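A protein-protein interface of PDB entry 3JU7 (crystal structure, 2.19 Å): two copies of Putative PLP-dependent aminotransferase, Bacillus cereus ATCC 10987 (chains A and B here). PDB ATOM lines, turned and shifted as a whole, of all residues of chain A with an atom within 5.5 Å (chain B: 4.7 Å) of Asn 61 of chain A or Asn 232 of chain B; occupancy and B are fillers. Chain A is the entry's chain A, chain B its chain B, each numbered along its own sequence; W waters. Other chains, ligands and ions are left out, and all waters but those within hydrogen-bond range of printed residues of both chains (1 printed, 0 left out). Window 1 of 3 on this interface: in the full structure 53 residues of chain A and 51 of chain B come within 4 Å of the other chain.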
ATOM      1  N   VAL A  59      24.003 -20.562   1.339  1.00  0.00           N
ATOM      2  CA  VAL A  59      24.192 -20.779   2.777  1.00  0.00           C
ATOM      3  C   VAL A  59      25.630 -21.248   2.986  1.00  0.00           C
ATOM      4  O   VAL A  59      26.295 -21.613   2.025  1.00  0.00           O
ATOM      5  CB  VAL A  59      23.202 -21.785   3.363  1.00  0.00           C
ATOM      6  CG1 VAL A  59      21.793 -21.196   3.324  1.00  0.00           C
ATOM      7  CG2 VAL A  59      23.281 -23.124   2.616  1.00  0.00           C
ATOM      8  N   ALA A  60      26.113 -21.261   4.232  1.00  0.00           N
ATOM      9  CA  ALA A  60      27.528 -21.518   4.469  1.00  0.00           C
ATOM     10  C   ALA A  60      27.879 -22.976   4.229  1.00  0.00           C
ATOM     11  O   ALA A  60      29.012 -23.295   3.886  1.00  0.00           O
ATOM     12  CB  ALA A  60      27.934 -21.067   5.844  1.00  0.00           C
ATOM     13  N   ASN A  61      26.895 -23.850   4.429  1.00  0.00           N
ATOM     14  CA  ASN A  61      26.969 -25.257   4.069  1.00  0.00           C
ATOM     15  C   ASN A  61      25.535 -25.850   4.054  1.00  0.00           C
ATOM     16  O   ASN A  61      24.589 -25.259   4.624  1.00  0.00           O
ATOM     17  CB  ASN A  61      27.961 -26.030   4.988  1.00  0.00           C
ATOM     18  CG  ASN A  61      27.490 -26.141   6.417  1.00  0.00           C
ATOM     19  OD1 ASN A  61      26.389 -26.664   6.680  1.00  0.00           O
ATOM     20  ND2 ASN A  61      28.343 -25.724   7.369  1.00  0.00           N
ATOM     21  N   ALA A  62      25.367 -26.980   3.382  1.00  0.00           N
ATOM     22  CA  ALA A  62      24.026 -27.617   3.203  1.00  0.00           C
ATOM     23  C   ALA A  62      23.451 -28.089   4.516  1.00  0.00           C
ATOM     24  O   ALA A  62      22.239 -28.133   4.664  1.00  0.00           O
ATOM     25  CB  ALA A  62      24.092 -28.807   2.236  1.00  0.00           C
ATOM     26  N   THR A  63      24.309 -28.464   5.467  1.00  0.00           N
ATOM     27  CA  THR A  63      23.789 -28.912   6.755  1.00  0.00           C
ATOM     28  C   THR A  63      23.019 -27.794   7.428  1.00  0.00           C
ATOM     29  O   THR A  63      21.879 -27.986   7.872  1.00  0.00           O
ATOM     30  CB  THR A  63      24.870 -29.481   7.655  1.00  0.00           C
ATOM     31  OG1 THR A  63      25.544 -30.496   6.912  1.00  0.00           O
ATOM     32  CG2 THR A  63      24.223 -30.055   8.942  1.00  0.00           C
ATOM     33  N   LEU A  64      23.613 -26.608   7.415  1.00  0.00           N
ATOM     34  CA  LEU A  64      22.958 -25.406   7.967  1.00  0.00           C
ATOM     35  C   LEU A  64      21.731 -24.991   7.141  1.00  0.00           C
ATOM     36  O   LEU A  64      20.744 -24.495   7.671  1.00  0.00           O
ATOM     37  CB  LEU A  64      23.929 -24.248   8.006  1.00  0.00           C
ATOM     38  CG  LEU A  64      25.158 -24.474   8.884  1.00  0.00           C
ATOM     39  CD1 LEU A  64      26.173 -23.386   8.521  1.00  0.00           C
ATOM     40  CD2 LEU A  64      24.793 -24.504  10.386  1.00  0.00           C
ATOM     41  N   GLY A  65      21.782 -25.213   5.848  1.00  0.00           N
ATOM     42  CA  GLY A  65      20.614 -24.953   5.024  1.00  0.00           C
ATOM     43  C   GLY A  65      19.481 -25.899   5.417  1.00  0.00           C
ATOM     44  O   GLY A  65      18.312 -25.498   5.498  1.00  0.00           O
ATOM     45  N   LEU A  66      19.811 -27.169   5.649  1.00  0.00           N
ATOM     46  CA  LEU A  66      18.802 -28.121   6.065  1.00  0.00           C
ATOM     47  C   LEU A  66      18.161 -27.604   7.339  1.00  0.00           C
ATOM     48  O   LEU A  66      16.903 -27.548   7.439  1.00  0.00           O
ATOM     49  CB  LEU A  66      19.367 -29.554   6.237  1.00  0.00           C
ATOM     50  CG  LEU A  66      19.417 -30.376   4.944  1.00  0.00           C
ATOM     51  CD1 LEU A  66      20.355 -31.575   5.070  1.00  0.00           C
ATOM     52  CD2 LEU A  66      18.014 -30.837   4.562  1.00  0.00           C
ATOM     53  N   HIS A 188      29.991 -28.456  -1.147  1.00  0.00           N
ATOM     54  CA  HIS A 188      31.206 -28.980  -0.537  1.00  0.00           C
ATOM     55  C   HIS A 188      32.181 -29.413  -1.633  1.00  0.00           C
ATOM     56  O   HIS A 188      31.759 -29.847  -2.716  1.00  0.00           O
ATOM     57  CB  HIS A 188      30.875 -30.153   0.366  1.00  0.00           C
ATOM     58  CG  HIS A 188      31.995 -30.583   1.254  1.00  0.00           C
ATOM     59  ND1 HIS A 188      32.802 -31.663   0.965  1.00  0.00           N
ATOM     60  CD2 HIS A 188      32.406 -30.120   2.464  1.00  0.00           C
ATOM     61  CE1 HIS A 188      33.672 -31.838   1.952  1.00  0.00           C
ATOM     62  NE2 HIS A 188      33.450 -30.918   2.877  1.00  0.00           N
ATOM     63  N1  LLP A 191      23.131 -34.329   3.053  1.00  0.00           N
ATOM     64  C2  LLP A 191      23.622 -35.169   2.089  1.00  0.00           C
ATOM     65  C2' LLP A 191      22.739 -36.203   1.490  1.00  0.00           C
ATOM     66  C3  LLP A 191      24.945 -35.034   1.682  1.00  0.00           C
ATOM     67  O3  LLP A 191      25.356 -35.806   0.821  1.00  0.00           O
ATOM     68  C4  LLP A 191      25.776 -34.032   2.240  1.00  0.00           C
ATOM     69  C4' LLP A 191      27.203 -33.869   1.804  1.00  0.00           C
ATOM     70  C5  LLP A 191      25.261 -33.183   3.211  1.00  0.00           C
ATOM     71  C6  LLP A 191      23.941 -33.346   3.597  1.00  0.00           C
ATOM     72  C5' LLP A 191      26.094 -32.085   3.854  1.00  0.00           C
ATOM     73  OP4 LLP A 191      26.474 -30.956   3.015  1.00  0.00           O
ATOM     74  P   LLP A 191      27.569 -29.889   3.481  1.00  0.00           P
ATOM     75  OP1 LLP A 191      27.204 -29.521   4.874  1.00  0.00           O
ATOM     76  OP2 LLP A 191      28.838 -30.642   3.374  1.00  0.00           O
ATOM     77  OP3 LLP A 191      27.525 -28.732   2.531  1.00  0.00           O
ATOM     78  N   LLP A 191      31.584 -32.691  -3.459  1.00  0.00           N
ATOM     79  CA  LLP A 191      30.397 -32.848  -4.274  1.00  0.00           C
ATOM     80  CB  LLP A 191      29.197 -32.081  -3.686  1.00  0.00           C
ATOM     81  CG  LLP A 191      29.006 -32.138  -2.180  1.00  0.00           C
ATOM     82  CD  LLP A 191      28.249 -33.321  -1.684  1.00  0.00           C
ATOM     83  CE  LLP A 191      28.411 -33.413  -0.163  1.00  0.00           C
ATOM     84  NZ  LLP A 191      27.255 -34.064   0.473  1.00  0.00           N
ATOM     85  C   LLP A 191      30.673 -32.323  -5.706  1.00  0.00           C
ATOM     86  O   LLP A 191      31.603 -31.565  -5.922  1.00  0.00           O
ATOM     87  N   GLU A 197      33.507 -25.053   1.035  1.00  0.00           N
ATOM     88  CA  GLU A 197      32.298 -25.142   1.843  1.00  0.00           C
ATOM     89  C   GLU A 197      31.240 -24.183   1.277  1.00  0.00           C
ATOM     90  O   GLU A 197      31.543 -23.055   0.872  1.00  0.00           O
ATOM     91  CB  GLU A 197      32.581 -24.793   3.292  1.00  0.00           C
ATOM     92  CG  GLU A 197      33.485 -25.784   4.014  1.00  0.00           C
ATOM     93  CD  GLU A 197      32.786 -27.060   4.488  1.00  0.00           C
ATOM     94  OE1 GLU A 197      31.540 -27.119   4.543  1.00  0.00           O
ATOM     95  OE2 GLU A 197      33.506 -28.011   4.851  1.00  0.00           O
ATOM     96  N   GLY A 198      30.011 -24.668   1.193  1.00  0.00           N
ATOM     97  CA  GLY A 198      28.915 -23.874   0.702  1.00  0.00           C
ATOM     98  C   GLY A 198      27.668 -24.716   0.455  1.00  0.00           C
ATOM     99  O   GLY A 198      27.699 -25.930   0.538  1.00  0.00           O
ATOM    100  N   GLY A 199      26.582 -24.050   0.129  1.00  0.00           N
ATOM    101  CA  GLY A 199      25.339 -24.698  -0.200  1.00  0.00           C
ATOM    102  C   GLY A 199      24.357 -23.683  -0.739  1.00  0.00           C
ATOM    103  O   GLY A 199      24.676 -22.490  -0.822  1.00  0.00           O
ATOM    104  N   CYS A 233      24.375 -18.440   8.954  1.00  0.00           N
ATOM    105  CA  CYS A 233      24.756 -19.392   7.910  1.00  0.00           C
ATOM    106  C   CYS A 233      25.044 -18.652   6.618  1.00  0.00           C
ATOM    107  O   CYS A 233      24.850 -19.192   5.546  1.00  0.00           O
ATOM    108  CB  CYS A 233      23.674 -20.452   7.702  1.00  0.00           C
ATOM    109  SG  CYS A 233      22.119 -19.800   6.943  1.00  0.00           S
ATOM    110  N   LEU B  64      28.231 -20.435  15.172  1.00  0.00           N
ATOM    111  CA  LEU B  64      28.302 -21.894  15.159  1.00  0.00           C
ATOM    112  C   LEU B  64      29.205 -22.385  16.268  1.00  0.00           C
ATOM    113  O   LEU B  64      28.961 -23.441  16.828  1.00  0.00           O
ATOM    114  CB  LEU B  64      28.810 -22.444  13.791  1.00  0.00           C
ATOM    115  CG  LEU B  64      27.957 -22.168  12.525  1.00  0.00           C
ATOM    116  CD1 LEU B  64      28.609 -22.709  11.268  1.00  0.00           C
ATOM    117  CD2 LEU B  64      26.556 -22.738  12.633  1.00  0.00           C
ATOM    118  N   GLY B 216      31.913 -30.724  14.886  1.00  0.00           N
ATOM    119  CA  GLY B 216      31.895 -29.902  13.674  1.00  0.00           C
ATOM    120  C   GLY B 216      31.962 -30.731  12.420  1.00  0.00           C
ATOM    121  O   GLY B 216      31.747 -30.193  11.305  1.00  0.00           O
ATOM    122  N   PHE B 218      29.964 -33.796  11.875  1.00  0.00           N
ATOM    123  CA  PHE B 218      28.870 -34.786  11.977  1.00  0.00           C
ATOM    124  C   PHE B 218      28.996 -35.770  13.137  1.00  0.00           C
ATOM    125  O   PHE B 218      28.373 -36.829  13.124  1.00  0.00           O
ATOM    126  CB  PHE B 218      28.718 -35.530  10.625  1.00  0.00           C
ATOM    127  CG  PHE B 218      28.686 -34.575   9.462  1.00  0.00           C
ATOM    128  CD1 PHE B 218      27.585 -33.757   9.265  1.00  0.00           C
ATOM    129  CD2 PHE B 218      29.780 -34.426   8.639  1.00  0.00           C
ATOM    130  CE1 PHE B 218      27.559 -32.814   8.237  1.00  0.00           C
ATOM    131  CE2 PHE B 218      29.765 -33.517   7.610  1.00  0.00           C
ATOM    132  CZ  PHE B 218      28.669 -32.698   7.417  1.00  0.00           C
ATOM    133  N   PHE B 231      27.161 -31.539  13.593  1.00  0.00           N
ATOM    134  CA  PHE B 231      26.655 -30.770  12.461  1.00  0.00           C
ATOM    135  C   PHE B 231      27.831 -30.458  11.570  1.00  0.00           C
ATOM    136  O   PHE B 231      28.830 -31.167  11.643  1.00  0.00           O
ATOM    137  CB  PHE B 231      25.774 -29.548  12.830  1.00  0.00           C
ATOM    138  CG  PHE B 231      26.407 -28.478  13.730  1.00  0.00           C
ATOM    139  CD1 PHE B 231      27.718 -28.507  14.172  1.00  0.00           C
ATOM    140  CD2 PHE B 231      25.635 -27.383  14.085  1.00  0.00           C
ATOM    141  CE1 PHE B 231      28.217 -27.482  15.011  1.00  0.00           C
ATOM    142  CE2 PHE B 231      26.141 -26.361  14.895  1.00  0.00           C
ATOM    143  CZ  PHE B 231      27.427 -26.409  15.343  1.00  0.00           C
ATOM    144  N   ASN B 232      27.739 -29.435  10.723  1.00  0.00           N
ATOM    145  CA  ASN B 232      28.898 -29.010   9.954  1.00  0.00           C
ATOM    146  C   ASN B 232      29.229 -27.572  10.371  1.00  0.00           C
ATOM    147  O   ASN B 232      28.412 -26.689  10.150  1.00  0.00           O
ATOM    148  CB  ASN B 232      28.575 -29.082   8.469  1.00  0.00           C
ATOM    149  CG  ASN B 232      29.707 -28.650   7.596  1.00  0.00           C
ATOM    150  OD1 ASN B 232      30.740 -28.203   8.081  1.00  0.00           O
ATOM    151  ND2 ASN B 232      29.521 -28.770   6.274  1.00  0.00           N
ATOM    152  N   CYS B 233      30.396 -27.331  10.984  1.00  0.00           N
ATOM    153  CA  CYS B 233      30.865 -25.950  11.147  1.00  0.00           C
ATOM    154  C   CYS B 233      32.326 -25.860  10.738  1.00  0.00           C
ATOM    155  O   CYS B 233      33.108 -25.070  11.282  1.00  0.00           O
ATOM    156  CB  CYS B 233      30.659 -25.439  12.560  1.00  0.00           C
ATOM    157  SG  CYS B 233      31.581 -26.396  13.781  1.00  0.00           S
ATOM    158  N   LYS B 234      32.676 -26.647   9.727  1.00  0.00           N
ATOM    159  CA  LYS B 234      34.036 -26.711   9.241  1.00  0.00           C
ATOM    160  C   LYS B 234      34.415 -25.426   8.510  1.00  0.00           C
ATOM    161  O   LYS B 234      33.662 -24.908   7.720  1.00  0.00           O
ATOM    162  CB  LYS B 234      34.238 -27.967   8.367  1.00  0.00           C
ATOM    163  CG  LYS B 234      34.189 -29.296   9.189  1.00  0.00           C
ATOM    164  CD  LYS B 234      34.192 -30.568   8.345  1.00  0.00           C
ATOM    165  CE  LYS B 234      32.840 -30.887   7.639  1.00  0.00           C
ATOM    166  NZ  LYS B 234      32.514 -29.888   6.553  1.00  0.00           N
HETATM  167  O   HOH W   1      31.039 -24.877   6.503  1.00  0.00           O
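OP1 of LLP 191 of chain A sits close to the side-chain amide nitrogen (ND2) of Asn 232 of chain B (2.8 Å).
The side-chain amino group (NZ) of Lys 234 of chain B lies within salt-bridge range of the side-chain carboxylate (OE2) of Glu 197 of chain A (2.7 Å).
The side-chain amide nitrogen of Asn 61 of chain A sits at hydrogen-bond distance from the backbone carbonyl oxygen of Asn 232 of chain B, 2.9 Å away.
ND2 of Asn 232 of chain B lies within hydrogen-bond range of OE1 of Glu 197 of chain A (3.1 Å).
OP3 of LLP 191 of chain A sits close to the backbone carbonyl oxygen (O) of Gly 198 of chain A, 3.4 Å away.
OP1 of LLP 191 of chain A lies close to the side-chain amide oxygen (OD1) of Asn 61 of chain A, at 3.5 Å.
OP3 of LLP 191 of chain A sits close to the backbone NH (N) of Ala 62 of chain A, at 2.9 Å.
The side-chain amide oxygen (OD1) of Asn 61 of chain A sits at hydrogen-bond distance from the backbone NH (N) of Leu 64 of chain A (2.9 Å).
NZ of Lys 234 of chain B lies within hydrogen-bond range of OD1 of Asn 232 of chain B (2.9 Å).
OP1 of LLP 191 of chain A lies close to the side-chain hydroxyl (OG1) of Thr 63 of chain A, at 2.8 Å.
OG1 of Thr 63 of chain A touches CE1 of Phe 218 of chain B, 3.3 Å away.
Thr 63 of chain A touches Asn 232 of chain B.
Leu 64 of chain A touches Leu 64 of chain B.
His 188 of chain A touches Lys 234 of chain B.
Printed residues of chain B within 4 Å of Asn 61 of chain A: Asn 232.
Printed residues of chain B within 4 Å of His 188 of chain A: Lys 234 (3.9 Å).
Of the printed residues of chain B, LLP 191 of chain A touches Asn 232 (2.8 Å).
Of chain A, only Asn 61 (2.9 Å), Thr 63 (3.7 Å), LLP 191 (2.8 Å) and Glu 197 (3.1 Å) come within 4 Å of Asn 232 of chain B.
Of the 14 printed residues of chain A, 6 touch a printed residue of chain B.
Printed residues of chain A that touch a printed residue of chain B: Asn 61, Thr 63, Leu 64, His 188, LLP 191 and Glu 197.
Hydrophobic or aromatic side chains of chain B that line the printed part of chain A: Leu 64 and Phe 218.
Along chain B the printed residues that touch a printed residue of chain A span positions 64 to 234.
Among the printed residues, Asp or Glu carboxylates within 4 Å of a Lys or Arg side-chain nitrogen of the other chain: Glu 197 of chain A with Lys 234 of chain B.
Leu 64 of chain A touches its own counterpart, Leu 64 of chain B.
2 positions are printed for both chains.
Water W1 lies within hydrogen-bond range of O of Lys 234 of chain B (2.9 Å), ND2 of Asn 61 of chain A (3.0 Å) and OE1 of Glu 197 of chain A (3.0 Å).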
